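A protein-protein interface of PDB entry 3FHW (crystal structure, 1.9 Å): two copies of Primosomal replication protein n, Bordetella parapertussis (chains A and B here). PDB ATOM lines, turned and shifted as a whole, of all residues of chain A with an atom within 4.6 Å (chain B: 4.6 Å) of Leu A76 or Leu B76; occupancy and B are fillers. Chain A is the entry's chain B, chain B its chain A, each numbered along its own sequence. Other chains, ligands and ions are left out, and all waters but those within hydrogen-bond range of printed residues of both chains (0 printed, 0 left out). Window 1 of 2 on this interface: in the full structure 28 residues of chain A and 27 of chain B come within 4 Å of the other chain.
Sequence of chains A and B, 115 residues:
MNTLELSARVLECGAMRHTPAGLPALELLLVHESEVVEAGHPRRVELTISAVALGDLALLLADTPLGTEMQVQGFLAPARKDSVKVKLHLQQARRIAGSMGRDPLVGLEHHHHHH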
ATOM      1  N   ASN A   2      11.114 -23.669   2.174  1.00  0.00           N
ATOM      2  CA  ASN A   2      11.313 -22.249   2.476  1.00  0.00           C
ATOM      3  C   ASN A   2      12.785 -21.907   2.255  1.00  0.00           C
ATOM      4  O   ASN A   2      13.601 -21.992   3.178  1.00  0.00           O
ATOM      5  CB  ASN A   2      10.890 -21.910   3.921  1.00  0.00           C
ATOM      6  CG  ASN A   2      11.085 -20.432   4.267  1.00  0.00           C
ATOM      7  OD1 ASN A   2      11.731 -19.687   3.521  1.00  0.00           O
ATOM      8  ND2 ASN A   2      10.528 -20.003   5.408  1.00  0.00           N
ATOM      9  N   LEU A   4      15.263 -19.061   0.035  1.00  0.00           N
ATOM     10  CA  LEU A   4      15.542 -17.930  -0.832  1.00  0.00           C
ATOM     11  C   LEU A   4      17.005 -17.968  -1.222  1.00  0.00           C
ATOM     12  O   LEU A   4      17.877 -18.088  -0.349  1.00  0.00           O
ATOM     13  CB  LEU A   4      15.265 -16.618  -0.099  1.00  0.00           C
ATOM     14  CG  LEU A   4      15.733 -15.322  -0.761  1.00  0.00           C
ATOM     15  CD1 LEU A   4      15.028 -15.094  -2.120  1.00  0.00           C
ATOM     16  CD2 LEU A   4      15.499 -14.130   0.184  1.00  0.00           C
ATOM     17  N   VAL A  45      14.350  -5.482 -10.689  1.00  0.00           N
ATOM     18  CA  VAL A  45      14.071  -5.630  -9.263  1.00  0.00           C
ATOM     19  C   VAL A  45      15.218  -5.045  -8.436  1.00  0.00           C
ATOM     20  O   VAL A  45      16.387  -5.321  -8.701  1.00  0.00           O
ATOM     21  CB  VAL A  45      13.714  -7.112  -8.865  1.00  0.00           C
ATOM     22  CG1 VAL A  45      14.720  -8.109  -9.428  1.00  0.00           C
ATOM     23  CG2 VAL A  45      13.609  -7.273  -7.351  1.00  0.00           C
ATOM     24  N   LEU A  47      15.942  -4.860  -4.319  1.00  0.00           N
ATOM     25  CA  LEU A  47      15.462  -5.334  -3.026  1.00  0.00           C
ATOM     26  C   LEU A  47      16.481  -5.115  -1.906  1.00  0.00           C
ATOM     27  O   LEU A  47      17.629  -5.531  -2.039  1.00  0.00           O
ATOM     28  CB  LEU A  47      15.143  -6.831  -3.133  1.00  0.00           C
ATOM     29  CG  LEU A  47      14.785  -7.604  -1.854  1.00  0.00           C
ATOM     30  CD1 LEU A  47      13.378  -7.260  -1.381  1.00  0.00           C
ATOM     31  CD2 LEU A  47      14.926  -9.116  -2.082  1.00  0.00           C
ATOM     32  N   ILE A  49      17.205  -6.119   2.065  1.00  0.00           N
ATOM     33  CA  ILE A  49      16.752  -7.119   3.034  1.00  0.00           C
ATOM     34  C   ILE A  49      17.763  -7.307   4.169  1.00  0.00           C
ATOM     35  O   ILE A  49      18.974  -7.369   3.924  1.00  0.00           O
ATOM     36  CB  ILE A  49      16.433  -8.472   2.327  1.00  0.00           C
ATOM     37  CG1 ILE A  49      15.740  -9.461   3.284  1.00  0.00           C
ATOM     38  CG2 ILE A  49      17.691  -9.078   1.676  1.00  0.00           C
ATOM     39  CD1 ILE A  49      14.912 -10.510   2.591  1.00  0.00           C
ATOM     40  N   GLY A  74      19.023 -18.982   2.295  1.00  0.00           N
ATOM     41  CA  GLY A  74      18.491 -19.302   3.624  1.00  0.00           C
ATOM     42  C   GLY A  74      16.985 -19.275   3.641  1.00  0.00           C
ATOM     43  O   GLY A  74      16.348 -19.215   2.587  1.00  0.00           O
ATOM     44  N   PHE A  75      16.412 -19.283   4.838  1.00  0.00           N
ATOM     45  CA  PHE A  75      14.955 -19.231   4.957  1.00  0.00           C
ATOM     46  C   PHE A  75      14.460 -17.853   5.373  1.00  0.00           C
ATOM     47  O   PHE A  75      15.146 -17.118   6.076  1.00  0.00           O
ATOM     48  CB  PHE A  75      14.410 -20.335   5.882  1.00  0.00           C
ATOM     49  CG  PHE A  75      14.827 -20.211   7.325  1.00  0.00           C
ATOM     50  CD1 PHE A  75      14.064 -19.453   8.221  1.00  0.00           C
ATOM     51  CD2 PHE A  75      15.954 -20.870   7.795  1.00  0.00           C
ATOM     52  CE1 PHE A  75      14.428 -19.346   9.558  1.00  0.00           C
ATOM     53  CE2 PHE A  75      16.337 -20.772   9.144  1.00  0.00           C
ATOM     54  CZ  PHE A  75      15.571 -20.006  10.022  1.00  0.00           C
ATOM     55  N   LEU A  76      13.248 -17.522   4.936  1.00  0.00           N
ATOM     56  CA  LEU A  76      12.610 -16.262   5.298  1.00  0.00           C
ATOM     57  C   LEU A  76      11.768 -16.402   6.551  1.00  0.00           C
ATOM     58  O   LEU A  76      11.117 -17.434   6.772  1.00  0.00           O
ATOM     59  CB  LEU A  76      11.720 -15.780   4.147  1.00  0.00           C
ATOM     60  CG  LEU A  76      12.359 -15.184   2.897  1.00  0.00           C
ATOM     61  CD1 LEU A  76      11.242 -14.794   1.949  1.00  0.00           C
ATOM     62  CD2 LEU A  76      13.224 -13.961   3.253  1.00  0.00           C
ATOM     63  N   ALA A  77      11.766 -15.354   7.372  1.00  0.00           N
ATOM     64  CA  ALA A  77      10.939 -15.326   8.555  1.00  0.00           C
ATOM     65  C   ALA A  77      10.603 -13.875   8.866  1.00  0.00           C
ATOM     66  O   ALA A  77      11.384 -12.980   8.531  1.00  0.00           O
ATOM     67  CB  ALA A  77      11.670 -15.974   9.741  1.00  0.00           C
ATOM     68  N   LYS A  87      13.122 -11.201   7.392  1.00  0.00           N
ATOM     69  CA  LYS A  87      14.552 -11.359   7.582  1.00  0.00           C
ATOM     70  C   LYS A  87      14.965 -12.676   6.968  1.00  0.00           C
ATOM     71  O   LYS A  87      14.281 -13.683   7.128  1.00  0.00           O
ATOM     72  CB  LYS A  87      14.941 -11.302   9.071  1.00  0.00           C
ATOM     73  CG  LYS A  87      15.284  -9.904   9.554  1.00  0.00           C
ATOM     74  CD  LYS A  87      15.572  -9.840  11.052  1.00  0.00           C
ATOM     75  CE  LYS A  87      16.883 -10.497  11.409  1.00  0.00           C
ATOM     76  NZ  LYS A  87      17.200 -10.376  12.865  1.00  0.00           N
ATOM     77  N   LEU A  88      16.068 -12.636   6.236  1.00  0.00           N
ATOM     78  CA  LEU A  88      16.664 -13.837   5.670  1.00  0.00           C
ATOM     79  C   LEU A  88      17.547 -14.457   6.734  1.00  0.00           C
ATOM     80  O   LEU A  88      18.507 -13.833   7.195  1.00  0.00           O
ATOM     81  CB  LEU A  88      17.487 -13.514   4.420  1.00  0.00           C
ATOM     82  CG  LEU A  88      18.292 -14.661   3.776  1.00  0.00           C
ATOM     83  CD1 LEU A  88      17.390 -15.815   3.404  1.00  0.00           C
ATOM     84  CD2 LEU A  88      19.080 -14.179   2.551  1.00  0.00           C
ATOM     85  N   ASN B   2      17.611 -14.456  -7.698  1.00  0.00           N
ATOM     86  CA  ASN B   2      16.515 -14.020  -6.829  1.00  0.00           C
ATOM     87  C   ASN B   2      15.376 -15.023  -6.990  1.00  0.00           C
ATOM     88  O   ASN B   2      14.532 -14.882  -7.877  1.00  0.00           O
ATOM     89  CB  ASN B   2      16.050 -12.588  -7.178  1.00  0.00           C
ATOM     90  CG  ASN B   2      14.959 -12.061  -6.244  1.00  0.00           C
ATOM     91  OD1 ASN B   2      14.349 -12.809  -5.474  1.00  0.00           O
ATOM     92  ND2 ASN B   2      14.694 -10.754  -6.329  1.00  0.00           N
ATOM     93  N   LEU B   4      12.717 -17.501  -4.542  1.00  0.00           N
ATOM     94  CA  LEU B   4      12.150 -18.054  -3.325  1.00  0.00           C
ATOM     95  C   LEU B   4      11.247 -19.217  -3.690  1.00  0.00           C
ATOM     96  O   LEU B   4      10.346 -19.056  -4.514  1.00  0.00           O
ATOM     97  CB  LEU B   4      11.310 -16.984  -2.617  1.00  0.00           C
ATOM     98  CG  LEU B   4      10.470 -17.428  -1.427  1.00  0.00           C
ATOM     99  CD1 LEU B   4      11.370 -17.940  -0.289  1.00  0.00           C
ATOM    100  CD2 LEU B   4       9.608 -16.265  -0.959  1.00  0.00           C
ATOM    101  N   VAL B  45       9.232 -21.940  11.774  1.00  0.00           N
ATOM    102  CA  VAL B  45       8.986 -20.668  11.124  1.00  0.00           C
ATOM    103  C   VAL B  45       7.510 -20.574  10.745  1.00  0.00           C
ATOM    104  O   VAL B  45       6.937 -21.531  10.225  1.00  0.00           O
ATOM    105  CB  VAL B  45       9.933 -20.445   9.894  1.00  0.00           C
ATOM    106  CG1 VAL B  45      10.046 -21.706   9.031  1.00  0.00           C
ATOM    107  CG2 VAL B  45       9.479 -19.248   9.051  1.00  0.00           C
ATOM    108  N   LEU B  47       5.357 -17.766   8.485  1.00  0.00           N
ATOM    109  CA  LEU B  47       5.570 -16.622   7.612  1.00  0.00           C
ATOM    110  C   LEU B  47       4.312 -16.330   6.814  1.00  0.00           C
ATOM    111  O   LEU B  47       3.817 -17.209   6.117  1.00  0.00           O
ATOM    112  CB  LEU B  47       6.739 -16.905   6.654  1.00  0.00           C
ATOM    113  CG  LEU B  47       7.014 -15.899   5.516  1.00  0.00           C
ATOM    114  CD1 LEU B  47       7.620 -14.577   6.038  1.00  0.00           C
ATOM    115  CD2 LEU B  47       7.902 -16.512   4.426  1.00  0.00           C
ATOM    116  N   ILE B  49       2.906 -13.954   3.760  1.00  0.00           N
ATOM    117  CA  ILE B  49       3.494 -13.205   2.646  1.00  0.00           C
ATOM    118  C   ILE B  49       2.491 -12.933   1.514  1.00  0.00           C
ATOM    119  O   ILE B  49       1.756 -13.838   1.087  1.00  0.00           O
ATOM    120  CB  ILE B  49       4.802 -13.897   2.110  1.00  0.00           C
ATOM    121  CG1 ILE B  49       5.532 -13.005   1.089  1.00  0.00           C
ATOM    122  CG2 ILE B  49       4.520 -15.323   1.552  1.00  0.00           C
ATOM    123  CD1 ILE B  49       6.996 -13.302   0.908  1.00  0.00           C
ATOM    124  N   GLY B  74       9.055 -17.938  -7.013  1.00  0.00           N
ATOM    125  CA  GLY B  74       9.161 -16.686  -7.769  1.00  0.00           C
ATOM    126  C   GLY B  74      10.284 -15.817  -7.246  1.00  0.00           C
ATOM    127  O   GLY B  74      11.174 -16.298  -6.539  1.00  0.00           O
ATOM    128  N   PHE B  75      10.233 -14.531  -7.575  1.00  0.00           N
ATOM    129  CA  PHE B  75      11.230 -13.593  -7.072  1.00  0.00           C
ATOM    130  C   PHE B  75      10.613 -12.652  -6.051  1.00  0.00           C
ATOM    131  O   PHE B  75       9.425 -12.375  -6.093  1.00  0.00           O
ATOM    132  CB  PHE B  75      11.940 -12.826  -8.204  1.00  0.00           C
ATOM    133  CG  PHE B  75      11.033 -11.938  -9.029  1.00  0.00           C
ATOM    134  CD1 PHE B  75      10.405 -12.434 -10.172  1.00  0.00           C
ATOM    135  CD2 PHE B  75      10.835 -10.600  -8.688  1.00  0.00           C
ATOM    136  CE1 PHE B  75       9.572 -11.621 -10.950  1.00  0.00           C
ATOM    137  CE2 PHE B  75      10.015  -9.779  -9.466  1.00  0.00           C
ATOM    138  CZ  PHE B  75       9.380 -10.297 -10.601  1.00  0.00           C
ATOM    139  N   LEU B  76      11.443 -12.162  -5.140  1.00  0.00           N
ATOM    140  CA  LEU B  76      11.021 -11.195  -4.132  1.00  0.00           C
ATOM    141  C   LEU B  76      11.257  -9.762  -4.581  1.00  0.00           C
ATOM    142  O   LEU B  76      12.253  -9.450  -5.268  1.00  0.00           O
ATOM    143  CB  LEU B  76      11.787 -11.427  -2.832  1.00  0.00           C
ATOM    144  CG  LEU B  76      11.417 -12.535  -1.867  1.00  0.00           C
ATOM    145  CD1 LEU B  76      12.317 -12.337  -0.645  1.00  0.00           C
ATOM    146  CD2 LEU B  76       9.922 -12.524  -1.463  1.00  0.00           C
ATOM    147  N   ALA B  77      10.335  -8.882  -4.190  1.00  0.00           N
ATOM    148  CA  ALA B  77      10.468  -7.468  -4.460  1.00  0.00           C
ATOM    149  C   ALA B  77       9.758  -6.694  -3.360  1.00  0.00           C
ATOM    150  O   ALA B  77       8.836  -7.214  -2.730  1.00  0.00           O
ATOM    151  CB  ALA B  77       9.877  -7.107  -5.830  1.00  0.00           C
ATOM    152  N   VAL B  86       7.493  -6.927   1.703  1.00  0.00           N
ATOM    153  CA  VAL B  86       7.869  -7.584   0.457  1.00  0.00           C
ATOM    154  C   VAL B  86       6.684  -8.307  -0.193  1.00  0.00           C
ATOM    155  O   VAL B  86       5.694  -8.658   0.473  1.00  0.00           O
ATOM    156  CB  VAL B  86       9.051  -8.568   0.644  1.00  0.00           C
ATOM    157  CG1 VAL B  86      10.313  -7.805   1.077  1.00  0.00           C
ATOM    158  CG2 VAL B  86       8.690  -9.672   1.645  1.00  0.00           C
ATOM    159  N   LYS B  87       6.782  -8.531  -1.501  1.00  0.00           N
ATOM    160  CA  LYS B  87       5.794  -9.367  -2.164  1.00  0.00           C
ATOM    161  C   LYS B  87       6.517 -10.389  -3.004  1.00  0.00           C
ATOM    162  O   LYS B  87       7.534 -10.086  -3.610  1.00  0.00           O
ATOM    163  CB  LYS B  87       4.823  -8.544  -3.016  1.00  0.00           C
ATOM    164  CG  LYS B  87       3.790  -7.791  -2.172  1.00  0.00           C
ATOM    165  CD  LYS B  87       2.959  -6.824  -2.994  1.00  0.00           C
ATOM    166  CE  LYS B  87       2.355  -7.498  -4.185  1.00  0.00           C
ATOM    167  NZ  LYS B  87       1.403  -6.599  -4.864  1.00  0.00           N
ATOM    168  N   LEU B  88       5.984 -11.603  -3.005  1.00  0.00           N
ATOM    169  CA  LEU B  88       6.506 -12.665  -3.859  1.00  0.00           C
ATOM    170  C   LEU B  88       5.890 -12.560  -5.238  1.00  0.00           C
ATOM    171  O   LEU B  88       4.687 -12.704  -5.392  1.00  0.00           O
ATOM    172  CB  LEU B  88       6.220 -14.044  -3.254  1.00  0.00           C
ATOM    173  CG  LEU B  88       6.578 -15.284  -4.092  1.00  0.00           C
ATOM    174  CD1 LEU B  88       8.034 -15.260  -4.478  1.00  0.00           C
ATOM    175  CD2 LEU B  88       6.257 -16.584  -3.367  1.00  0.00           C
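ND2 of Asn A2 touches CG2 of Val B45 (3.9 Å). Asn B2 touches Val A45. Leu B76 touches Val A45. Leu B76 touches Leu A47. Leu A47 touches Val B86 (CD1 to CG1, 3.97 Å). CD1 of Leu A76 touches CD2 of Leu B4, 3.6 Å away. Val B45 touches Leu A76. Leu A76 touches Leu B47. CD1 of Leu A76 touches CD1 of Leu B76 (3.7 Å). CG2 of Val B45 touches CB of Ala A77, 3.999 Å away.
Leu A76 touches four residues of chain B. Printed residues of chain A within 4 Å of Leu B76: Leu A4, Val A45, Leu A47 and Leu A76. Printed residues of chain B within 4 Å of Val A45: Asn B2 and Leu B76. Printed residues of chain A within 4 Å of Leu B47: Leu A76 (3.9 Å). Of the printed residues of chain A, Val B45 touches Asn A2, Leu A76 and Ala A77.
Printed residues of chain B that touch a printed residue of chain A: Asn B2, Leu B4, Val B45, Leu B47, Leu B76 and Val B86. Hydrophobic or aromatic side chains of chain A within 4 Å of the printed part of chain B: Leu A4, Val A45, Leu A47, Leu A76 and Ala A77. Among the printed residues, no Asp or Glu carboxylate lies within 4 Å of a Lys or Arg side-chain nitrogen of the other chain.
Asn A2 touches Val B45, and with the chains exchanged Val A45 touches Asn B2. Leu A4 touches Leu B76, and with the chains exchanged Leu A76 touches Leu B4. Val A45 touches Leu B76, and with the chains exchanged Leu A76 touches Val B45. Leu A47 touches Leu B76, and with the chains exchanged Leu A76 touches Leu B47. Of the 11 pairs that touch across the chains among the printed residues, 9 have their exchanged pair printed and touching as well.
N of Leu A4 sits at hydrogen-bond distance from O of Gly A74. The backbone carbonyl oxygen (O) of Leu B76 sits at hydrogen-bond distance from the side-chain amide nitrogen (ND2) of Asn B2. The backbone carbonyl oxygen (O) of Leu A76 lies within hydrogen-bond range of the side-chain amide nitrogen (ND2) of Asn A2, 3.0 Å away. N of Lys A87 sits at hydrogen-bond distance from O of Ala A77 (2.7 Å). O of Gly B74 lies within hydrogen-bond range of N of Leu B4, at 2.8 Å.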
